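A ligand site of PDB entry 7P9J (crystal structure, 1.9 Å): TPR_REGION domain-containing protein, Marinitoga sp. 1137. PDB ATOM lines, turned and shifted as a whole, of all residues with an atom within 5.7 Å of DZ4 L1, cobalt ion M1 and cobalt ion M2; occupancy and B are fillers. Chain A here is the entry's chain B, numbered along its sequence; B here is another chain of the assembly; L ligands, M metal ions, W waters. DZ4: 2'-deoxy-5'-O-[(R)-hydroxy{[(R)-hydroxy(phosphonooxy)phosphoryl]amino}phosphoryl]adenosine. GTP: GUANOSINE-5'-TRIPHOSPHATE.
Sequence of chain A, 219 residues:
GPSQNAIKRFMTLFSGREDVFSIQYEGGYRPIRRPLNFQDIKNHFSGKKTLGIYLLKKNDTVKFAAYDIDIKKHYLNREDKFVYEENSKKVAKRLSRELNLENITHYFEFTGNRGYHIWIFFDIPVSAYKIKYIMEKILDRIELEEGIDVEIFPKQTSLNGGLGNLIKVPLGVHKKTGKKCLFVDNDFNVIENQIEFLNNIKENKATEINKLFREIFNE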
ATOM      1  N   GLY A  27      -3.165  -7.764 -11.574  1.00  0.00           N
ATOM      2  CA  GLY A  27      -2.263  -7.819 -10.401  1.00  0.00           C
ATOM      3  C   GLY A  27      -0.871  -7.296 -10.716  1.00  0.00           C
ATOM      4  O   GLY A  27      -0.040  -7.329  -9.803  1.00  0.00           O
ATOM      5  N   GLY A  28      -0.621  -6.814 -11.923  1.00  0.00           N
ATOM      6  CA  GLY A  28       0.720  -6.234 -12.155  1.00  0.00           C
ATOM      7  C   GLY A  28       1.070  -6.092 -13.618  1.00  0.00           C
ATOM      8  O   GLY A  28       0.153  -6.051 -14.451  1.00  0.00           O
ATOM      9  N   TYR A  29       2.368  -5.964 -13.907  1.00  0.00           N
ATOM     10  CA  TYR A  29       2.851  -5.861 -15.293  1.00  0.00           C
ATOM     11  C   TYR A  29       4.008  -6.850 -15.475  1.00  0.00           C
ATOM     12  O   TYR A  29       4.713  -7.122 -14.501  1.00  0.00           O
ATOM     13  CB  TYR A  29       3.279  -4.427 -15.618  1.00  0.00           C
ATOM     14  CG  TYR A  29       2.179  -3.446 -15.899  1.00  0.00           C
ATOM     15  CD1 TYR A  29       1.430  -2.905 -14.872  1.00  0.00           C
ATOM     16  CD2 TYR A  29       1.909  -3.020 -17.193  1.00  0.00           C
ATOM     17  CE1 TYR A  29       0.411  -1.994 -15.106  1.00  0.00           C
ATOM     18  CE2 TYR A  29       0.903  -2.096 -17.453  1.00  0.00           C
ATOM     19  CZ  TYR A  29       0.154  -1.585 -16.405  1.00  0.00           C
ATOM     20  OH  TYR A  29      -0.832  -0.689 -16.641  1.00  0.00           O
ATOM     21  N   ASP A  68       0.921  11.948 -15.468  1.00  0.00           N
ATOM     22  CA  ASP A  68      -0.047  11.006 -14.913  1.00  0.00           C
ATOM     23  C   ASP A  68      -0.800  11.613 -13.719  1.00  0.00           C
ATOM     24  O   ASP A  68      -0.267  11.668 -12.601  1.00  0.00           O
ATOM     25  CB  ASP A  68       0.662   9.711 -14.524  1.00  0.00           C
ATOM     26  CG  ASP A  68      -0.253   8.724 -13.829  1.00  0.00           C
ATOM     27  OD1 ASP A  68      -1.436   8.601 -14.240  1.00  0.00           O
ATOM     28  OD2 ASP A  68       0.230   8.033 -12.910  1.00  0.00           O
ATOM     29  N   ILE A  69      -2.032  12.057 -13.961  1.00  0.00           N
ATOM     30  CA  ILE A  69      -2.860  12.655 -12.921  1.00  0.00           C
ATOM     31  C   ILE A  69      -3.754  11.582 -12.301  1.00  0.00           C
ATOM     32  O   ILE A  69      -4.569  10.960 -12.999  1.00  0.00           O
ATOM     33  CB  ILE A  69      -3.693  13.825 -13.462  1.00  0.00           C
ATOM     34  CG1 ILE A  69      -2.774  14.917 -14.006  1.00  0.00           C
ATOM     35  CG2 ILE A  69      -4.572  14.411 -12.356  1.00  0.00           C
ATOM     36  CD1 ILE A  69      -2.880  15.150 -15.487  1.00  0.00           C
ATOM     37  N   ASP A  70      -3.613  11.389 -10.995  1.00  0.00           N
ATOM     38  CA  ASP A  70      -4.248  10.305 -10.261  1.00  0.00           C
ATOM     39  C   ASP A  70      -5.154  10.883  -9.173  1.00  0.00           C
ATOM     40  O   ASP A  70      -4.713  11.706  -8.375  1.00  0.00           O
ATOM     41  CB  ASP A  70      -3.188   9.446  -9.577  1.00  0.00           C
ATOM     42  CG  ASP A  70      -2.638   8.372 -10.464  1.00  0.00           C
ATOM     43  OD1 ASP A  70      -2.683   8.513 -11.704  1.00  0.00           O
ATOM     44  OD2 ASP A  70      -2.077   7.419  -9.901  1.00  0.00           O
ATOM     45  N   LYS A  72      -6.205   9.955  -5.856  1.00  0.00           N
ATOM     46  CA  LYS A  72      -5.725   9.022  -4.817  1.00  0.00           C
ATOM     47  C   LYS A  72      -6.885   8.303  -4.109  1.00  0.00           C
ATOM     48  O   LYS A  72      -8.047   8.672  -4.351  1.00  0.00           O
ATOM     49  CB  LYS A  72      -4.838   9.761  -3.825  1.00  0.00           C
ATOM     50  CG  LYS A  72      -3.401   9.973  -4.270  1.00  0.00           C
ATOM     51  CD  LYS A  72      -2.867   8.882  -5.176  1.00  0.00           C
ATOM     52  CE  LYS A  72      -1.480   8.419  -4.814  1.00  0.00           C
ATOM     53  NZ  LYS A  72      -0.681   8.060  -6.012  1.00  0.00           N
ATOM     54  N   THR A 111      -7.730   7.336 -18.674  1.00  0.00           N
ATOM     55  CA  THR A 111      -6.908   6.133 -18.419  1.00  0.00           C
ATOM     56  C   THR A 111      -7.677   4.824 -18.205  1.00  0.00           C
ATOM     57  O   THR A 111      -7.008   3.803 -18.068  1.00  0.00           O
ATOM     58  CB  THR A 111      -5.982   6.416 -17.237  1.00  0.00           C
ATOM     59  OG1 THR A 111      -6.762   6.661 -16.073  1.00  0.00           O
ATOM     60  CG2 THR A 111      -5.120   7.610 -17.562  1.00  0.00           C
ATOM     61  N   GLY A 112      -8.993   4.864 -18.165  1.00  0.00           N
ATOM     62  CA  GLY A 112      -9.787   3.652 -17.990  1.00  0.00           C
ATOM     63  C   GLY A 112     -10.175   3.424 -16.545  1.00  0.00           C
ATOM     64  O   GLY A 112     -10.920   2.498 -16.304  1.00  0.00           O
ATOM     65  N   ASN A 113      -9.696   4.271 -15.625  1.00  0.00           N
ATOM     66  CA  ASN A 113      -9.974   4.062 -14.180  1.00  0.00           C
ATOM     67  C   ASN A 113     -10.063   5.375 -13.401  1.00  0.00           C
ATOM     68  O   ASN A 113     -11.183   5.869 -13.241  1.00  0.00           O
ATOM     69  CB  ASN A 113      -8.930   3.139 -13.536  1.00  0.00           C
ATOM     70  CG  ASN A 113      -9.204   2.786 -12.083  1.00  0.00           C
ATOM     71  OD1 ASN A 113     -10.338   2.775 -11.629  1.00  0.00           O
ATOM     72  ND2 ASN A 113      -8.142   2.492 -11.346  1.00  0.00           N
ATOM     73  N   ARG A 114      -8.925   5.911 -12.928  1.00  0.00           N
ATOM     74  CA  ARG A 114      -8.969   7.070 -12.010  1.00  0.00           C
ATOM     75  C   ARG A 114      -8.198   8.296 -12.485  1.00  0.00           C
ATOM     76  O   ARG A 114      -7.607   8.988 -11.646  1.00  0.00           O
ATOM     77  CB  ARG A 114      -8.422   6.623 -10.648  1.00  0.00           C
ATOM     78  CG  ARG A 114      -7.098   5.874 -10.702  1.00  0.00           C
ATOM     79  CD  ARG A 114      -6.036   6.508  -9.839  1.00  0.00           C
ATOM     80  NE  ARG A 114      -4.793   5.756  -9.893  1.00  0.00           N
ATOM     81  CZ  ARG A 114      -4.134   5.315  -8.841  1.00  0.00           C
ATOM     82  NH1 ARG A 114      -4.578   5.565  -7.622  1.00  0.00           N
ATOM     83  NH2 ARG A 114      -3.015   4.636  -9.000  1.00  0.00           N
ATOM     84  N   GLY A 115      -8.211   8.589 -13.769  1.00  0.00           N
ATOM     85  CA  GLY A 115      -7.516   9.834 -14.104  1.00  0.00           C
ATOM     86  C   GLY A 115      -7.201  10.070 -15.544  1.00  0.00           C
ATOM     87  O   GLY A 115      -7.858   9.477 -16.417  1.00  0.00           O
ATOM     88  N   HIS A 117      -4.000  10.885 -18.536  1.00  0.00           N
ATOM     89  CA  HIS A 117      -2.624  11.083 -18.972  1.00  0.00           C
ATOM     90  C   HIS A 117      -2.594  12.269 -19.934  1.00  0.00           C
ATOM     91  O   HIS A 117      -3.477  12.410 -20.787  1.00  0.00           O
ATOM     92  CB  HIS A 117      -2.074   9.849 -19.696  1.00  0.00           C
ATOM     93  CG  HIS A 117      -1.940   8.623 -18.839  1.00  0.00           C
ATOM     94  ND1 HIS A 117      -1.990   7.353 -19.368  1.00  0.00           N
ATOM     95  CD2 HIS A 117      -1.756   8.460 -17.504  1.00  0.00           C
ATOM     96  CE1 HIS A 117      -1.858   6.454 -18.401  1.00  0.00           C
ATOM     97  NE2 HIS A 117      -1.710   7.107 -17.263  1.00  0.00           N
ATOM     98  N   ASP A 149      -2.838  13.339  -7.293  1.00  0.00           N
ATOM     99  CA  ASP A 149      -1.370  13.149  -7.354  1.00  0.00           C
ATOM    100  C   ASP A 149      -0.943  13.394  -8.798  1.00  0.00           C
ATOM    101  O   ASP A 149      -1.716  13.063  -9.698  1.00  0.00           O
ATOM    102  CB  ASP A 149      -0.985  11.753  -6.849  1.00  0.00           C
ATOM    103  CG  ASP A 149       0.142  11.063  -7.598  1.00  0.00           C
ATOM    104  OD1 ASP A 149      -0.149  10.357  -8.579  1.00  0.00           O
ATOM    105  OD2 ASP A 149       1.308  11.234  -7.181  1.00  0.00           O
ATOM    106  N   GLU A 151       2.162  12.528 -11.459  1.00  0.00           N
ATOM    107  CA  GLU A 151       3.431  11.806 -11.693  1.00  0.00           C
ATOM    108  C   GLU A 151       3.989  12.216 -13.055  1.00  0.00           C
ATOM    109  O   GLU A 151       3.210  12.515 -13.962  1.00  0.00           O
ATOM    110  CB  GLU A 151       3.219  10.308 -11.585  1.00  0.00           C
ATOM    111  CG  GLU A 151       3.121   9.805 -10.172  1.00  0.00           C
ATOM    112  CD  GLU A 151       2.677   8.362 -10.113  1.00  0.00           C
ATOM    113  OE1 GLU A 151       3.532   7.486 -10.330  1.00  0.00           O
ATOM    114  OE2 GLU A 151       1.483   8.124  -9.888  1.00  0.00           O
ATOM    115  N   PHE A 153       6.341  11.024 -16.254  1.00  0.00           N
ATOM    116  CA  PHE A 153       7.009   9.945 -16.988  1.00  0.00           C
ATOM    117  C   PHE A 153       7.793  10.573 -18.136  1.00  0.00           C
ATOM    118  O   PHE A 153       7.176  11.242 -18.973  1.00  0.00           O
ATOM    119  CB  PHE A 153       5.973   8.956 -17.534  1.00  0.00           C
ATOM    120  CG  PHE A 153       5.412   8.040 -16.496  1.00  0.00           C
ATOM    121  CD1 PHE A 153       4.415   8.483 -15.636  1.00  0.00           C
ATOM    122  CD2 PHE A 153       5.861   6.726 -16.374  1.00  0.00           C
ATOM    123  CE1 PHE A 153       3.895   7.664 -14.663  1.00  0.00           C
ATOM    124  CE2 PHE A 153       5.349   5.904 -15.390  1.00  0.00           C
ATOM    125  CZ  PHE A 153       4.351   6.373 -14.541  1.00  0.00           C
ATOM    126  N   ASN A 165      10.996   2.913 -16.254  1.00  0.00           N
ATOM    127  CA  ASN A 165       9.576   2.800 -15.974  1.00  0.00           C
ATOM    128  C   ASN A 165       8.778   2.834 -17.273  1.00  0.00           C
ATOM    129  O   ASN A 165       9.204   3.426 -18.263  1.00  0.00           O
ATOM    130  CB  ASN A 165       9.104   3.905 -15.022  1.00  0.00           C
ATOM    131  CG  ASN A 165       9.349   3.552 -13.561  1.00  0.00           C
ATOM    132  OD1 ASN A 165      10.449   3.722 -13.055  1.00  0.00           O
ATOM    133  ND2 ASN A 165       8.321   3.063 -12.885  1.00  0.00           N
ATOM    134  N   LEU A 166       7.620   2.175 -17.235  1.00  0.00           N
ATOM    135  CA  LEU A 166       6.718   2.045 -18.352  1.00  0.00           C
ATOM    136  C   LEU A 166       5.391   2.703 -18.031  1.00  0.00           C
ATOM    137  O   LEU A 166       5.041   2.911 -16.861  1.00  0.00           O
ATOM    138  CB  LEU A 166       6.488   0.565 -18.694  1.00  0.00           C
ATOM    139  CG  LEU A 166       5.716  -0.094 -17.546  1.00  0.00           C
ATOM    140  CD1 LEU A 166       4.255  -0.349 -17.848  1.00  0.00           C
ATOM    141  CD2 LEU A 166       6.436  -1.370 -17.115  1.00  0.00           C
ATOM    142  N   ILE A 167       4.619   2.962 -19.084  1.00  0.00           N
ATOM    143  CA  ILE A 167       3.285   3.535 -18.973  1.00  0.00           C
ATOM    144  C   ILE A 167       2.348   2.771 -19.894  1.00  0.00           C
ATOM    145  O   ILE A 167       2.717   2.423 -21.030  1.00  0.00           O
ATOM    146  CB  ILE A 167       3.297   5.038 -19.298  1.00  0.00           C
ATOM    147  CG1 ILE A 167       1.932   5.672 -19.046  1.00  0.00           C
ATOM    148  CG2 ILE A 167       3.763   5.288 -20.736  1.00  0.00           C
ATOM    149  CD1 ILE A 167       1.974   7.202 -18.945  1.00  0.00           C
ATOM    150  N   LYS A 168       1.143   2.492 -19.393  1.00  0.00           N
ATOM    151  CA  LYS A 168       0.088   1.865 -20.241  1.00  0.00           C
ATOM    152  C   LYS A 168      -0.267   2.862 -21.337  1.00  0.00           C
ATOM    153  O   LYS A 168      -0.518   4.033 -21.025  1.00  0.00           O
ATOM    154  CB  LYS A 168      -1.138   1.467 -19.412  1.00  0.00           C
ATOM    155  CG  LYS A 168      -2.326   0.945 -20.201  1.00  0.00           C
ATOM    156  CD  LYS A 168      -3.489   0.497 -19.352  1.00  0.00           C
ATOM    157  CE  LYS A 168      -3.811   1.423 -18.204  1.00  0.00           C
ATOM    158  NZ  LYS A 168      -4.219   2.772 -18.654  1.00  0.00           N
ATOM    159  N   HIS A 174      -8.175  -1.273 -19.811  1.00  0.00           N
ATOM    160  CA  HIS A 174      -7.672  -1.318 -18.445  1.00  0.00           C
ATOM    161  C   HIS A 174      -8.164  -2.589 -17.780  1.00  0.00           C
ATOM    162  O   HIS A 174      -9.353  -2.715 -17.476  1.00  0.00           O
ATOM    163  CB  HIS A 174      -8.150  -0.082 -17.668  1.00  0.00           C
ATOM    164  CG  HIS A 174      -7.293   0.280 -16.496  1.00  0.00           C
ATOM    165  ND1 HIS A 174      -6.840  -0.660 -15.593  1.00  0.00           N
ATOM    166  CD2 HIS A 174      -6.867   1.478 -16.037  1.00  0.00           C
ATOM    167  CE1 HIS A 174      -6.123  -0.059 -14.656  1.00  0.00           C
ATOM    168  NE2 HIS A 174      -6.131   1.238 -14.905  1.00  0.00           N
ATOM    169  P    DT B   6       7.634 -12.183 -10.781  1.00  0.00           P
ATOM    170  OP1  DT B   6       8.285 -13.488 -10.533  1.00  0.00           O
ATOM    171  OP2  DT B   6       7.039 -11.424  -9.658  1.00  0.00           O
ATOM    172  O5'  DT B   6       8.686 -11.251 -11.525  1.00  0.00           O
ATOM    173  C5'  DT B   6       8.859 -11.342 -12.940  1.00  0.00           C
ATOM    174  C4'  DT B   6       9.224  -9.988 -13.511  1.00  0.00           C
ATOM    175  O4'  DT B   6       8.085  -9.094 -13.441  1.00  0.00           O
ATOM    176  C3'  DT B   6      10.373  -9.270 -12.799  1.00  0.00           C
ATOM    177  O3'  DT B   6      11.280  -8.778 -13.792  1.00  0.00           O
ATOM    178  C2'  DT B   6       9.686  -8.153 -12.031  1.00  0.00           C
ATOM    179  C1'  DT B   6       8.483  -7.853 -12.903  1.00  0.00           C
ATOM    180  N1   DT B   6       7.334  -7.285 -12.185  1.00  0.00           N
ATOM    181  C2   DT B   6       6.896  -6.027 -12.524  1.00  0.00           C
ATOM    182  O2   DT B   6       7.424  -5.346 -13.389  1.00  0.00           O
ATOM    183  N3   DT B   6       5.796  -5.605 -11.825  1.00  0.00           N
ATOM    184  C4   DT B   6       5.115  -6.284 -10.837  1.00  0.00           C
ATOM    185  O4   DT B   6       4.153  -5.770 -10.291  1.00  0.00           O
ATOM    186  C5   DT B   6       5.636  -7.601 -10.534  1.00  0.00           C
ATOM    187  C7   DT B   6       4.958  -8.417  -9.470  1.00  0.00           C
ATOM    188  C6   DT B   6       6.703  -8.024 -11.215  1.00  0.00           C
ATOM    189  P    DC B   7      12.761  -8.381 -13.398  1.00  0.00           P
ATOM    190  OP1  DC B   7      13.623  -8.580 -14.588  1.00  0.00           O
ATOM    191  OP2  DC B   7      13.111  -9.036 -12.122  1.00  0.00           O
ATOM    192  O5'  DC B   7      12.664  -6.806 -13.165  1.00  0.00           O
ATOM    193  C5'  DC B   7      12.129  -5.954 -14.189  1.00  0.00           C
ATOM    194  C4'  DC B   7      11.817  -4.580 -13.641  1.00  0.00           C
ATOM    195  O4'  DC B   7      10.577  -4.622 -12.897  1.00  0.00           O
ATOM    196  C3'  DC B   7      12.872  -4.027 -12.682  1.00  0.00           C
ATOM    197  O3'  DC B   7      13.386  -2.821 -13.251  1.00  0.00           O
ATOM    198  C2'  DC B   7      12.100  -3.778 -11.384  1.00  0.00           C
ATOM    199  C1'  DC B   7      10.669  -3.681 -11.856  1.00  0.00           C
ATOM    200  N1   DC B   7       9.662  -4.023 -10.847  1.00  0.00           N
ATOM    201  C2   DC B   7       8.566  -3.175 -10.693  1.00  0.00           C
ATOM    202  O2   DC B   7       8.473  -2.171 -11.406  1.00  0.00           O
ATOM    203  N3   DC B   7       7.619  -3.475  -9.768  1.00  0.00           N
ATOM    204  C4   DC B   7       7.757  -4.575  -9.012  1.00  0.00           C
ATOM    205  N4   DC B   7       6.810  -4.832  -8.114  1.00  0.00           N
ATOM    206  C5   DC B   7       8.865  -5.457  -9.157  1.00  0.00           C
ATOM    207  C6   DC B   7       9.796  -5.134 -10.063  1.00  0.00           C
HETATM  208  N1  DZ4 L   1       4.808  -2.620 -12.620  1.00  0.00           N
HETATM  209  C2  DZ4 L   1       5.257  -1.803 -13.592  1.00  0.00           C
HETATM  210  N3  DZ4 L   1       4.735  -0.640 -14.033  1.00  0.00           N
HETATM  211  C4  DZ4 L   1       3.642  -0.353 -13.346  1.00  0.00           C
HETATM  212  C5  DZ4 L   1       3.076  -1.126 -12.316  1.00  0.00           C
HETATM  213  C6  DZ4 L   1       3.719  -2.263 -12.001  1.00  0.00           C
HETATM  214  N6  DZ4 L   1       3.174  -3.086 -10.945  1.00  0.00           N
HETATM  215  N7  DZ4 L   1       1.835  -0.416 -11.812  1.00  0.00           N
HETATM  216  C8  DZ4 L   1       1.829   0.670 -12.612  1.00  0.00           C
HETATM  217  N9  DZ4 L   1       2.832   0.626 -13.408  1.00  0.00           N
HETATM  218  PA  DZ4 L   1      -1.081   3.965 -12.474  1.00  0.00           P
HETATM  219  PB  DZ4 L   1      -2.658   4.114 -14.993  1.00  0.00           P
HETATM  220  PG  DZ4 L   1      -5.090   4.502 -13.614  1.00  0.00           P
HETATM  221  C1' DZ4 L   1       3.056   1.631 -14.375  1.00  0.00           C
HETATM  222  O1A DZ4 L   1      -1.406   5.338 -12.155  1.00  0.00           O
HETATM  223  O1B DZ4 L   1      -2.133   3.617 -16.236  1.00  0.00           O
HETATM  224  O1G DZ4 L   1      -4.317   5.311 -12.716  1.00  0.00           O
HETATM  225  C2' DZ4 L   1       2.070   1.391 -15.525  1.00  0.00           C
HETATM  226  O2A DZ4 L   1      -1.314   3.319 -11.200  1.00  0.00           O
HETATM  227  O2B DZ4 L   1      -2.195   5.471 -14.987  1.00  0.00           O
HETATM  228  O2G DZ4 L   1      -6.268   5.290 -13.852  1.00  0.00           O
HETATM  229  C3' DZ4 L   1       1.129   2.522 -15.390  1.00  0.00           C
HETATM  230  O3' DZ4 L   1       0.571   2.903 -16.639  1.00  0.00           O
HETATM  231  N3A DZ4 L   1      -2.073   3.257 -13.650  1.00  0.00           N
HETATM  232  O3B DZ4 L   1      -4.288   4.074 -14.969  1.00  0.00           O
HETATM  233  O3G DZ4 L   1      -5.556   3.415 -12.796  1.00  0.00           O
HETATM  234  C4' DZ4 L   1       1.918   3.616 -14.777  1.00  0.00           C
HETATM  235  O4' DZ4 L   1       2.880   3.005 -13.908  1.00  0.00           O
HETATM  236  C5' DZ4 L   1       0.976   4.508 -13.990  1.00  0.00           C
HETATM  237  O5' DZ4 L   1       0.486   3.802 -12.902  1.00  0.00           O
HETATM  238  PG  GTP L   2      -3.202   4.895  -3.547  1.00  0.00           P
HETATM  239  O1G GTP L   2      -2.759   6.016  -2.650  1.00  0.00           O
HETATM  240  O2G GTP L   2      -4.088   5.363  -4.660  1.00  0.00           O
HETATM  241  O3G GTP L   2      -3.796   3.751  -2.779  1.00  0.00           O
HETATM  242  O3B GTP L   2      -1.862   4.302  -4.230  1.00  0.00           O
HETATM  243  PB  GTP L   2      -1.446   3.982  -5.730  1.00  0.00           P
HETATM  244  O1B GTP L   2      -2.290   2.861  -6.241  1.00  0.00           O
HETATM  245  O2B GTP L   2      -1.385   5.252  -6.502  1.00  0.00           O
HETATM  246  O3A GTP L   2       0.040   3.442  -5.549  1.00  0.00           O
HETATM  247  PA  GTP L   2       1.291   3.991  -4.720  1.00  0.00           P
HETATM  248  O1A GTP L   2       0.943   5.297  -4.095  1.00  0.00           O
HETATM  249  O2A GTP L   2       1.785   2.896  -3.843  1.00  0.00           O
HETATM  250  O5' GTP L   2       2.356   4.233  -5.893  1.00  0.00           O
HETATM  251  C5' GTP L   2       2.334   5.506  -6.597  1.00  0.00           C
HETATM  252  C4' GTP L   2       2.514   5.269  -8.081  1.00  0.00           C
HETATM  253  O4' GTP L   2       3.637   4.377  -8.304  1.00  0.00           O
HETATM  254  C3' GTP L   2       1.341   4.624  -8.821  1.00  0.00           C
HETATM  255  O3' GTP L   2       0.372   5.592  -9.210  1.00  0.00           O
HETATM  256  C2' GTP L   2       2.055   4.013 -10.022  1.00  0.00           C
HETATM  257  O2' GTP L   2       2.349   4.972 -11.010  1.00  0.00           O
HETATM  258  C1' GTP L   2       3.382   3.558  -9.425  1.00  0.00           C
HETATM  259  N9  GTP L   2       3.423   2.155  -8.998  1.00  0.00           N
HETATM  260  C8  GTP L   2       2.590   1.519  -8.108  1.00  0.00           C
HETATM  261  N7  GTP L   2       2.900   0.267  -7.924  1.00  0.00           N
HETATM  262  C5  GTP L   2       4.004   0.060  -8.730  1.00  0.00           C
HETATM  263  C6  GTP L   2       4.778  -1.103  -8.942  1.00  0.00           C
HETATM  264  O6  GTP L   2       4.640  -2.225  -8.423  1.00  0.00           O
HETATM  265  N1  GTP L   2       5.812  -0.880  -9.854  1.00  0.00           N
HETATM  266  C2  GTP L   2       6.068   0.320 -10.468  1.00  0.00           C
HETATM  267  N2  GTP L   2       7.102   0.343 -11.309  1.00  0.00           N
HETATM  268  N3  GTP L   2       5.347   1.414 -10.278  1.00  0.00           N
HETATM  269  C4  GTP L   2       4.336   1.220  -9.404  1.00  0.00           C
HETATM  270 CO    CO M   1      -2.681   6.897 -13.234  1.00  0.00          CO
HETATM  271 CO    CO M   2      -0.025   6.887 -11.048  1.00  0.00          CO
HETATM  272  O   HOH W   1      -2.090   0.346 -14.099  1.00  0.00           O
HETATM  273  O   HOH W   2      -4.240   8.217 -14.725  1.00  0.00           O
HETATM  274  O   HOH W   3      -4.232   1.744 -11.258  1.00  0.00           O
HETATM  275  O   HOH W   4       5.630   3.366 -12.592  1.00  0.00           O
HETATM  276  O   HOH W   5       7.331   1.263 -14.892  1.00  0.00           O
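Merely in contact with DZ4 L1: Leu 166 (3.4 Å), Tyr 29 (3.5 Å), Ile 167 (3.6 Å), Phe 153 (3.7 Å), Gly 115 (3.8 Å) and DC 7 of chain B (3.9 Å). The nearest printed residue that does not touch DZ4 L1 is Gly 28 (4.2 Å).
An oxygen (O2G) of GTP L2 is in salt-bridge range of the guanidinium group of Arg 114 (3.0 Å). NE2 of His 174 sits at hydrogen-bond distance from O3G of DZ4 L1, at 3.1 Å. O4 of DT 6 of chain B sits at hydrogen-bond distance from a nitrogen (N6) of DZ4 L1 (2.9 Å). The side-chain amide nitrogen (ND2) of Asn 113 sits at hydrogen-bond distance from an oxygen (O3G) of DZ4 L1, 3.1 Å away. N2 of GTP L2 sits close to ND2 of Asn 165 (3.4 Å). NH2 of Arg 114 is in salt-bridge range of O2A of DZ4 L1 (3.1 Å). NE2 of His 117 lies close to O2B of DZ4 L1, 2.8 Å away. N of Lys 168 lies within hydrogen-bond range of O3' of DZ4 L1 (2.8 Å). An oxygen (O1B) of DZ4 L1 lies within salt-bridge range of the side-chain amino group (NZ) of Lys 168 (3.3 Å). N of Arg 114 sits at hydrogen-bond distance from O2G of DZ4 L1 (2.9 Å). OG1 of Thr 111 lies within hydrogen-bond range of O2G of DZ4 L1 (2.7 Å). O2 of DC 7 of chain B lies within hydrogen-bond range of a nitrogen (N2) of GTP L2. NZ of Lys 72 is in salt-bridge range of O2B of GTP L2 (2.9 Å).
Cobalt ion M2 is bound by OD2 of Asp 68 (2.2 Å), OE2 of Glu 151 (2.3 Å), O3' of GTP L2 (2.3 Å), O1A of DZ4 L1 (2.4 Å) and OD2 of Asp 70 (2.4 Å). Cobalt ion M2 has five donor atoms within binding distance.
Water W2 bridges the side-chain hydroxyl of Thr 111 (3.3 Å) and the backbone carbonyl oxygen of Ile 69 (3.3 Å). Water W1 lies within hydrogen-bond range of N3A of DZ4 L1 and OH of Tyr 29. Water W4 lies within hydrogen-bond range of ND2 of Asn 165, N3 of GTP L2 and O4' of DZ4 L1. Water W5 lies within hydrogen-bond range of N of Leu 166 (2.5 Å), ND2 of Asn 165 (2.9 Å) and N3 of DZ4 L1 (3.3 Å).
Cobalt ion M1 is bound by the side-chain carboxylate (OD1) of Asp 70, an oxygen (O1A) of DZ4 L1, an oxygen (O2B) of DZ4 L1, an oxygen (O1G) of DZ4 L1, the side-chain carboxylate (OD1) of Asp 68 and water W2.
The backbone carbonyl oxygen (O) of Asp 70 lies within hydrogen-bond range of the backbone NH (N) of Asp 149 (2.7 Å). O of Gly 115 lies within hydrogen-bond range of OG1 of Thr 111 (3.0 Å). The side-chain carboxylate (OD1) of Asp 68 lies close to a ring nitrogen (NE2) of His 117 (3.4 Å). OD2 of Asp 70 sits close to NH2 of Arg 114, 3.1 Å away. The backbone carbonyl oxygen (O) of Thr 111 lies within hydrogen-bond range of the side-chain amino group (NZ) of Lys 168, 3.0 Å away.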
